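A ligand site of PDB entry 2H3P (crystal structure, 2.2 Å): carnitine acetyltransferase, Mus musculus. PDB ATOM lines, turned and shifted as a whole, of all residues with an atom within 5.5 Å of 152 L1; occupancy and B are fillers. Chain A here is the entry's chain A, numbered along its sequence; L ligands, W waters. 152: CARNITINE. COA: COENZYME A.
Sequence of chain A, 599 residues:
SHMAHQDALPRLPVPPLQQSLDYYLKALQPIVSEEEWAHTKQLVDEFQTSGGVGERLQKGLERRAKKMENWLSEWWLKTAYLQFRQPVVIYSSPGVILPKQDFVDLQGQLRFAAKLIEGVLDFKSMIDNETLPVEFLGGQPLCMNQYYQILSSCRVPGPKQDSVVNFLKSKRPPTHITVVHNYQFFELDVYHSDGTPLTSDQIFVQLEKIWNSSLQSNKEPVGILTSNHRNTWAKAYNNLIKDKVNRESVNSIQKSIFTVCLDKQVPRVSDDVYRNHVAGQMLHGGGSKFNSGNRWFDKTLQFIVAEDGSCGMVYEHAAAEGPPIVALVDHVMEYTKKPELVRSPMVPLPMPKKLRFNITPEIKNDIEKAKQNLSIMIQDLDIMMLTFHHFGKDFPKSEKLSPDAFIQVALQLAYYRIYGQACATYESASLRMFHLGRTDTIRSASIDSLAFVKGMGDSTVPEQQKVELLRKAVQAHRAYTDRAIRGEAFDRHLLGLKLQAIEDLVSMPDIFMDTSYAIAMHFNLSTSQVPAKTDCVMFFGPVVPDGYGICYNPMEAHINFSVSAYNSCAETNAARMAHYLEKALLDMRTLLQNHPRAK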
ATOM      1  N   TRP A  76     -18.158   7.361  12.149  1.00  0.00           N
ATOM      2  CA  TRP A  76     -17.750   7.007  10.782  1.00  0.00           C
ATOM      3  C   TRP A  76     -18.114   8.088   9.776  1.00  0.00           C
ATOM      4  O   TRP A  76     -17.269   8.498   8.977  1.00  0.00           O
ATOM      5  CB  TRP A  76     -18.405   5.697  10.343  1.00  0.00           C
ATOM      6  CG  TRP A  76     -17.972   5.262   8.969  1.00  0.00           C
ATOM      7  CD1 TRP A  76     -18.755   5.115   7.850  1.00  0.00           C
ATOM      8  CD2 TRP A  76     -16.645   4.902   8.575  1.00  0.00           C
ATOM      9  NE1 TRP A  76     -17.988   4.670   6.795  1.00  0.00           N
ATOM     10  CE2 TRP A  76     -16.692   4.522   7.213  1.00  0.00           C
ATOM     11  CE3 TRP A  76     -15.411   4.839   9.248  1.00  0.00           C
ATOM     12  CZ2 TRP A  76     -15.555   4.106   6.502  1.00  0.00           C
ATOM     13  CZ3 TRP A  76     -14.277   4.415   8.541  1.00  0.00           C
ATOM     14  CH2 TRP A  76     -14.364   4.058   7.177  1.00  0.00           C
ATOM     15  N   TYR A  81     -16.192  11.055   5.970  1.00  0.00           N
ATOM     16  CA  TYR A  81     -16.636  12.021   4.970  1.00  0.00           C
ATOM     17  C   TYR A  81     -16.703  13.489   5.391  1.00  0.00           C
ATOM     18  O   TYR A  81     -16.025  14.346   4.827  1.00  0.00           O
ATOM     19  CB  TYR A  81     -18.007  11.599   4.411  1.00  0.00           C
ATOM     20  CG  TYR A  81     -18.049  10.171   3.917  1.00  0.00           C
ATOM     21  CD1 TYR A  81     -18.548   9.145   4.722  1.00  0.00           C
ATOM     22  CD2 TYR A  81     -17.509   9.825   2.680  1.00  0.00           C
ATOM     23  CE1 TYR A  81     -18.517   7.814   4.298  1.00  0.00           C
ATOM     24  CE2 TYR A  81     -17.470   8.490   2.251  1.00  0.00           C
ATOM     25  CZ  TYR A  81     -17.971   7.501   3.059  1.00  0.00           C
ATOM     26  OH  TYR A  81     -17.886   6.192   2.639  1.00  0.00           O
ATOM     27  N   PRO A  94     -18.016   8.543  -5.707  1.00  0.00           N
ATOM     28  CA  PRO A  94     -17.768   7.524  -6.719  1.00  0.00           C
ATOM     29  C   PRO A  94     -18.456   7.821  -8.050  1.00  0.00           C
ATOM     30  O   PRO A  94     -19.516   8.446  -8.084  1.00  0.00           O
ATOM     31  CB  PRO A  94     -18.312   6.243  -6.085  1.00  0.00           C
ATOM     32  CG  PRO A  94     -18.309   6.538  -4.598  1.00  0.00           C
ATOM     33  CD  PRO A  94     -18.765   7.970  -4.568  1.00  0.00           C
ATOM     34  N   TYR A 315     -22.255  10.044  -7.349  1.00  0.00           N
ATOM     35  CA  TYR A 315     -23.026  10.322  -6.148  1.00  0.00           C
ATOM     36  C   TYR A 315     -22.157  10.708  -4.975  1.00  0.00           C
ATOM     37  O   TYR A 315     -21.011  10.277  -4.859  1.00  0.00           O
ATOM     38  CB  TYR A 315     -23.877   9.106  -5.780  1.00  0.00           C
ATOM     39  CG  TYR A 315     -23.120   7.984  -5.113  1.00  0.00           C
ATOM     40  CD1 TYR A 315     -23.047   7.888  -3.726  1.00  0.00           C
ATOM     41  CD2 TYR A 315     -22.483   7.007  -5.877  1.00  0.00           C
ATOM     42  CE1 TYR A 315     -22.353   6.839  -3.111  1.00  0.00           C
ATOM     43  CE2 TYR A 315     -21.801   5.953  -5.277  1.00  0.00           C
ATOM     44  CZ  TYR A 315     -21.737   5.877  -3.903  1.00  0.00           C
ATOM     45  OH  TYR A 315     -21.061   4.821  -3.311  1.00  0.00           O
ATOM     46  N   HIS A 317     -20.796  10.354  -1.613  1.00  0.00           N
ATOM     47  CA  HIS A 317     -20.599   9.199  -0.729  1.00  0.00           C
ATOM     48  C   HIS A 317     -21.095   9.269   0.717  1.00  0.00           C
ATOM     49  O   HIS A 317     -21.246   8.240   1.361  1.00  0.00           O
ATOM     50  CB  HIS A 317     -19.117   8.829  -0.707  1.00  0.00           C
ATOM     51  CG  HIS A 317     -18.861   7.351  -0.673  1.00  0.00           C
ATOM     52  ND1 HIS A 317     -19.720   6.462  -0.051  1.00  0.00           N
ATOM     53  CD2 HIS A 317     -17.837   6.605  -1.143  1.00  0.00           C
ATOM     54  CE1 HIS A 317     -19.228   5.241  -0.149  1.00  0.00           C
ATOM     55  NE2 HIS A 317     -18.090   5.296  -0.813  1.00  0.00           N
ATOM     56  N   GLU A 321     -23.579   3.745   0.385  1.00  0.00           N
ATOM     57  CA  GLU A 321     -22.581   2.956  -0.311  1.00  0.00           C
ATOM     58  C   GLU A 321     -23.103   2.610  -1.697  1.00  0.00           C
ATOM     59  O   GLU A 321     -24.159   3.096  -2.119  1.00  0.00           O
ATOM     60  CB  GLU A 321     -22.266   1.663   0.448  1.00  0.00           C
ATOM     61  CG  GLU A 321     -20.985   1.750   1.272  1.00  0.00           C
ATOM     62  CD  GLU A 321     -21.104   2.759   2.382  1.00  0.00           C
ATOM     63  OE1 GLU A 321     -21.854   2.487   3.337  1.00  0.00           O
ATOM     64  OE2 GLU A 321     -20.463   3.821   2.287  1.00  0.00           O
ATOM     65  N   TYR A 426      -7.493  -2.953   1.314  1.00  0.00           N
ATOM     66  CA  TYR A 426      -8.803  -2.668   1.861  1.00  0.00           C
ATOM     67  C   TYR A 426      -9.894  -3.101   0.871  1.00  0.00           C
ATOM     68  O   TYR A 426      -9.796  -2.814  -0.329  1.00  0.00           O
ATOM     69  CB  TYR A 426      -8.920  -1.169   2.117  1.00  0.00           C
ATOM     70  CG  TYR A 426     -10.268  -0.671   2.601  1.00  0.00           C
ATOM     71  CD1 TYR A 426     -10.435  -0.232   3.913  1.00  0.00           C
ATOM     72  CD2 TYR A 426     -11.372  -0.629   1.745  1.00  0.00           C
ATOM     73  CE1 TYR A 426     -11.665   0.244   4.378  1.00  0.00           C
ATOM     74  CE2 TYR A 426     -12.613  -0.158   2.195  1.00  0.00           C
ATOM     75  CZ  TYR A 426     -12.745   0.272   3.508  1.00  0.00           C
ATOM     76  OH  TYR A 426     -13.967   0.727   3.962  1.00  0.00           O
ATOM     77  N   SER A 428     -14.206  -3.086   0.786  1.00  0.00           N
ATOM     78  CA  SER A 428     -15.460  -2.701   1.441  1.00  0.00           C
ATOM     79  C   SER A 428     -16.324  -3.891   1.850  1.00  0.00           C
ATOM     80  O   SER A 428     -16.597  -4.776   1.039  1.00  0.00           O
ATOM     81  CB  SER A 428     -16.293  -1.803   0.513  1.00  0.00           C
ATOM     82  OG  SER A 428     -15.659  -0.564   0.264  1.00  0.00           O
ATOM     83  N   ALA A 429     -16.759  -3.907   3.107  1.00  0.00           N
ATOM     84  CA  ALA A 429     -17.641  -4.958   3.590  1.00  0.00           C
ATOM     85  C   ALA A 429     -18.894  -4.264   4.122  1.00  0.00           C
ATOM     86  O   ALA A 429     -18.792  -3.317   4.888  1.00  0.00           O
ATOM     87  CB  ALA A 429     -16.968  -5.773   4.692  1.00  0.00           C
ATOM     88  N   THR A 439     -20.233   0.239   6.704  1.00  0.00           N
ATOM     89  CA  THR A 439     -19.182  -0.678   6.279  1.00  0.00           C
ATOM     90  C   THR A 439     -18.136  -1.014   7.323  1.00  0.00           C
ATOM     91  O   THR A 439     -18.016  -0.360   8.362  1.00  0.00           O
ATOM     92  CB  THR A 439     -18.372  -0.113   5.096  1.00  0.00           C
ATOM     93  OG1 THR A 439     -17.540   0.956   5.553  1.00  0.00           O
ATOM     94  CG2 THR A 439     -19.296   0.384   4.026  1.00  0.00           C
ATOM     95  N   ASP A 440     -17.380  -2.059   7.021  1.00  0.00           N
ATOM     96  CA  ASP A 440     -16.273  -2.464   7.858  1.00  0.00           C
ATOM     97  C   ASP A 440     -15.168  -2.852   6.877  1.00  0.00           C
ATOM     98  O   ASP A 440     -15.373  -2.843   5.670  1.00  0.00           O
ATOM     99  CB  ASP A 440     -16.614  -3.656   8.750  1.00  0.00           C
ATOM    100  CG  ASP A 440     -15.872  -3.612  10.088  1.00  0.00           C
ATOM    101  OD1 ASP A 440     -14.650  -3.355  10.086  1.00  0.00           O
ATOM    102  OD2 ASP A 440     -16.509  -3.823  11.132  1.00  0.00           O
ATOM    103  N   ARG A 492     -12.994  -1.136  12.173  1.00  0.00           N
ATOM    104  CA  ARG A 492     -13.898  -0.138  12.720  1.00  0.00           C
ATOM    105  C   ARG A 492     -13.794  -0.159  14.241  1.00  0.00           C
ATOM    106  O   ARG A 492     -13.929   0.876  14.889  1.00  0.00           O
ATOM    107  CB  ARG A 492     -15.339  -0.418  12.299  1.00  0.00           C
ATOM    108  CG  ARG A 492     -15.589  -0.302  10.808  1.00  0.00           C
ATOM    109  CD  ARG A 492     -15.418   1.131  10.294  1.00  0.00           C
ATOM    110  NE  ARG A 492     -15.561   1.154   8.841  1.00  0.00           N
ATOM    111  CZ  ARG A 492     -14.611   0.746   7.998  1.00  0.00           C
ATOM    112  NH1 ARG A 492     -13.453   0.294   8.474  1.00  0.00           N
ATOM    113  NH2 ARG A 492     -14.820   0.759   6.689  1.00  0.00           N
ATOM    114  N   SER A 526      -6.985  -0.014  -2.429  1.00  0.00           N
ATOM    115  CA  SER A 526      -8.283   0.284  -1.830  1.00  0.00           C
ATOM    116  C   SER A 526      -9.281  -0.219  -2.855  1.00  0.00           C
ATOM    117  O   SER A 526      -9.336   0.283  -3.981  1.00  0.00           O
ATOM    118  CB  SER A 526      -8.462   1.789  -1.619  1.00  0.00           C
ATOM    119  OG  SER A 526      -9.784   2.068  -1.177  1.00  0.00           O
ATOM    120  N   THR A 527     -10.086  -1.196  -2.454  1.00  0.00           N
ATOM    121  CA  THR A 527     -11.022  -1.833  -3.368  1.00  0.00           C
ATOM    122  C   THR A 527     -12.438  -2.030  -2.836  1.00  0.00           C
ATOM    123  O   THR A 527     -12.732  -1.832  -1.650  1.00  0.00           O
ATOM    124  CB  THR A 527     -10.518  -3.221  -3.747  1.00  0.00           C
ATOM    125  OG1 THR A 527     -10.740  -4.120  -2.662  1.00  0.00           O
ATOM    126  CG2 THR A 527      -9.021  -3.163  -4.013  1.00  0.00           C
ATOM    127  N   SER A 528     -13.329  -2.444  -3.725  1.00  0.00           N
ATOM    128  CA  SER A 528     -14.707  -2.727  -3.376  1.00  0.00           C
ATOM    129  C   SER A 528     -15.384  -3.441  -4.528  1.00  0.00           C
ATOM    130  O   SER A 528     -14.933  -3.380  -5.669  1.00  0.00           O
ATOM    131  CB  SER A 528     -15.486  -1.447  -3.065  1.00  0.00           C
ATOM    132  OG  SER A 528     -15.828  -0.763  -4.249  1.00  0.00           O
ATOM    133  N   PHE A 540     -13.398   5.070  -8.405  1.00  0.00           N
ATOM    134  CA  PHE A 540     -13.050   6.123  -7.457  1.00  0.00           C
ATOM    135  C   PHE A 540     -11.530   6.247  -7.436  1.00  0.00           C
ATOM    136  O   PHE A 540     -10.828   5.309  -7.809  1.00  0.00           O
ATOM    137  CB  PHE A 540     -13.575   5.763  -6.062  1.00  0.00           C
ATOM    138  CG  PHE A 540     -13.225   4.380  -5.625  1.00  0.00           C
ATOM    139  CD1 PHE A 540     -11.964   4.098  -5.126  1.00  0.00           C
ATOM    140  CD2 PHE A 540     -14.140   3.337  -5.755  1.00  0.00           C
ATOM    141  CE1 PHE A 540     -11.609   2.799  -4.770  1.00  0.00           C
ATOM    142  CE2 PHE A 540     -13.794   2.027  -5.402  1.00  0.00           C
ATOM    143  CZ  PHE A 540     -12.522   1.765  -4.904  1.00  0.00           C
ATOM    144  N   VAL A 543      -6.946   6.024  -2.272  1.00  0.00           N
ATOM    145  CA  VAL A 543      -7.067   6.709  -0.981  1.00  0.00           C
ATOM    146  C   VAL A 543      -5.715   7.244  -0.507  1.00  0.00           C
ATOM    147  O   VAL A 543      -5.657   8.077   0.394  1.00  0.00           O
ATOM    148  CB  VAL A 543      -7.697   5.788   0.098  1.00  0.00           C
ATOM    149  CG1 VAL A 543      -9.056   5.272  -0.388  1.00  0.00           C
ATOM    150  CG2 VAL A 543      -6.778   4.610   0.401  1.00  0.00           C
HETATM  151  C1  152 L   1     -16.397   2.207   2.385  1.00  0.00           C
HETATM  152  O1A 152 L   1     -16.649   2.702   3.511  1.00  0.00           O
HETATM  153  O1B 152 L   1     -15.814   1.097   2.236  1.00  0.00           O
HETATM  154  C2  152 L   1     -16.808   2.978   1.148  1.00  0.00           C
HETATM  155  C3  152 L   1     -15.880   2.732  -0.039  1.00  0.00           C
HETATM  156  O3  152 L   1     -16.612   3.043  -1.237  1.00  0.00           O
HETATM  157  C4  152 L   1     -14.673   3.691   0.075  1.00  0.00           C
HETATM  158  N5  152 L   1     -13.574   3.273  -0.814  1.00  0.00           N
HETATM  159  C5A 152 L   1     -13.370   1.827  -0.725  1.00  0.00           C
HETATM  160  C5B 152 L   1     -13.889   3.638  -2.204  1.00  0.00           C
HETATM  161  C5C 152 L   1     -12.352   3.953  -0.403  1.00  0.00           C
HETATM  162  N1A COA L   2     -19.120 -22.319  -4.554  1.00  0.00           N
HETATM  163  C2A COA L   2     -20.055 -21.983  -5.449  1.00  0.00           C
HETATM  164  N3A COA L   2     -20.612 -20.773  -5.428  1.00  0.00           N
HETATM  165  C4A COA L   2     -20.212 -19.830  -4.524  1.00  0.00           C
HETATM  166  C5A COA L   2     -19.250 -20.162  -3.586  1.00  0.00           C
HETATM  167  C6A COA L   2     -18.680 -21.428  -3.638  1.00  0.00           C
HETATM  168  N6A COA L   2     -17.716 -21.767  -2.778  1.00  0.00           N
HETATM  169  N7A COA L   2     -19.043 -19.090  -2.835  1.00  0.00           N
HETATM  170  C8A COA L   2     -19.870 -18.121  -3.258  1.00  0.00           C
HETATM  171  N9A COA L   2     -20.586 -18.583  -4.291  1.00  0.00           N
HETATM  172  C1B COA L   2     -21.579 -17.813  -5.110  1.00  0.00           C
HETATM  173  C2B COA L   2     -22.551 -17.012  -4.268  1.00  0.00           C
HETATM  174  O2B COA L   2     -23.627 -17.882  -3.862  1.00  0.00           O
HETATM  175  C3B COA L   2     -23.049 -15.998  -5.255  1.00  0.00           C
HETATM  176  O3B COA L   2     -23.988 -16.636  -6.128  1.00  0.00           O
HETATM  177  P3B COA L   2     -24.869 -15.765  -7.154  1.00  0.00           P
HETATM  178  O7A COA L   2     -26.087 -16.747  -7.512  1.00  0.00           O
HETATM  179  O8A COA L   2     -25.370 -14.584  -6.415  1.00  0.00           O
HETATM  180  O9A COA L   2     -24.068 -15.553  -8.388  1.00  0.00           O
HETATM  181  C4B COA L   2     -21.791 -15.624  -6.046  1.00  0.00           C
HETATM  182  O4B COA L   2     -20.939 -16.824  -5.972  1.00  0.00           O
HETATM  183  C5B COA L   2     -21.038 -14.448  -5.408  1.00  0.00           C
HETATM  184  O5B COA L   2     -20.628 -14.762  -4.067  1.00  0.00           O
HETATM  185  P1A COA L   2     -19.251 -14.147  -3.495  1.00  0.00           P
HETATM  186  O1A COA L   2     -18.289 -14.038  -4.613  1.00  0.00           O
HETATM  187  O2A COA L   2     -18.844 -14.897  -2.288  1.00  0.00           O
HETATM  188  O3A COA L   2     -19.676 -12.637  -3.085  1.00  0.00           O
HETATM  189  P2A COA L   2     -20.831 -12.336  -1.987  1.00  0.00           P
HETATM  190  O4A COA L   2     -20.697 -13.239  -0.822  1.00  0.00           O
HETATM  191  O5A COA L   2     -22.140 -12.258  -2.672  1.00  0.00           O
HETATM  192  O6A COA L   2     -20.439 -10.870  -1.513  1.00  0.00           O
HETATM  193  CBP COA L   2     -19.132  -9.167  -0.399  1.00  0.00           C
HETATM  194  CCP COA L   2     -19.258 -10.648  -0.734  1.00  0.00           C
HETATM  195  CDP COA L   2     -19.083  -8.362  -1.711  1.00  0.00           C
HETATM  196  CEP COA L   2     -17.830  -8.920   0.384  1.00  0.00           C
HETATM  197  CAP COA L   2     -20.373  -8.744   0.442  1.00  0.00           C
HETATM  198  OAP COA L   2     -20.440  -9.543   1.624  1.00  0.00           O
HETATM  199  C9P COA L   2     -20.330  -7.264   0.815  1.00  0.00           C
HETATM  200  O9P COA L   2     -19.833  -6.887   1.874  1.00  0.00           O
HETATM  201  N8P COA L   2     -20.865  -6.461  -0.104  1.00  0.00           N
HETATM  202  C7P COA L   2     -20.921  -5.008   0.056  1.00  0.00           C
HETATM  203  C6P COA L   2     -19.702  -4.328  -0.581  1.00  0.00           C
HETATM  204  C5P COA L   2     -19.926  -2.830  -0.671  1.00  0.00           C
HETATM  205  O5P COA L   2     -20.369  -2.199   0.299  1.00  0.00           O
HETATM  206  N4P COA L   2     -19.622  -2.288  -1.850  1.00  0.00           N
HETATM  207  C3P COA L   2     -19.793  -0.848  -2.170  1.00  0.00           C
HETATM  208  C2P COA L   2     -18.791   0.025  -1.392  1.00  0.00           C
HETATM  209  S1P COA L   2     -19.102   1.806  -1.659  1.00  0.00           S
HETATM  210  O   HOH W   1     -13.464   3.516   3.640  1.00  0.00           O
HETATM  211  O   HOH W   2     -17.072   1.890  -3.999  1.00  0.00           O
HETATM  212  O   HOH W   3     -14.381   6.822  -2.409  1.00  0.00           O
HETATM  213  O   HOH W   4     -14.905   5.544   2.731  1.00  0.00           O
HETATM  214  O   HOH W   5     -18.708   4.318   3.981  1.00  0.00           O
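An oxygen (O3) of 152 L1 sits close to a sulfur (S1P) of COA L2 (2.8 Å).
Water W5 lies within hydrogen-bond range of OH of Tyr 81 (2.4 Å), OE2 of Glu 321 (2.5 Å), O1A of 152 L1 (2.7 Å) and NE1 of Trp 76 (2.9 Å).
Water W2 lies within hydrogen-bond range of the side-chain hydroxyl (OG) of Ser 528 (2.9 Å), an oxygen (O3) of 152 L1 (3.0 Å) and a sulfur (S1P) of COA L2 (3.1 Å).
Water W4 bridges the side-chain hydroxyl (OH) of Tyr 81 (3.1 Å) and an oxygen (O1A) of 152 L1 (3.4 Å).
Water W1 bridges OH of Tyr 426 and O1A of 152 L1.
Residues that only touch 152 L1: Trp 76 (3.5 Å), Tyr 81 (3.7 Å), Glu 321 (3.9 Å), Ser 526 (3.3 Å), Thr 527 (3.8 Å), Phe 540 (3.5 Å) and Val 543 (3.6 Å).
Along chain A the residues within 4 Å of 152 L1 span positions 76 to 543.
O of Tyr 426 sits at hydrogen-bond distance from N of Thr 527, at 2.7 Å.
OH of Tyr 426 is in hydrogen-bond range of NH2 of Arg 492.
The backbone NH (N) of Ser 428 is in hydrogen-bond range of the backbone carbonyl oxygen (O) of Thr 527, 3.1 Å away.
A ring nitrogen (ND1) of His 317 lies close to the side-chain hydroxyl (OH) of Tyr 81 (3.3 Å).
O of Thr 439 sits at hydrogen-bond distance from NE of Arg 492.
An oxygen (O1B) of 152 L1 lies within hydrogen-bond range of the side-chain hydroxyl (OH) of Tyr 426 (2.6 Å).
OG of Ser 428 sits at hydrogen-bond distance from O1B of 152 L1 (2.6 Å).
O3 of 152 L1 lies within hydrogen-bond range of NE2 of His 317 (2.7 Å).
OG1 of Thr 439 sits at hydrogen-bond distance from O1A of 152 L1, at 2.8 Å.
S1P of COA L2 sits close to NE2 of His 317, 3.7 Å away.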
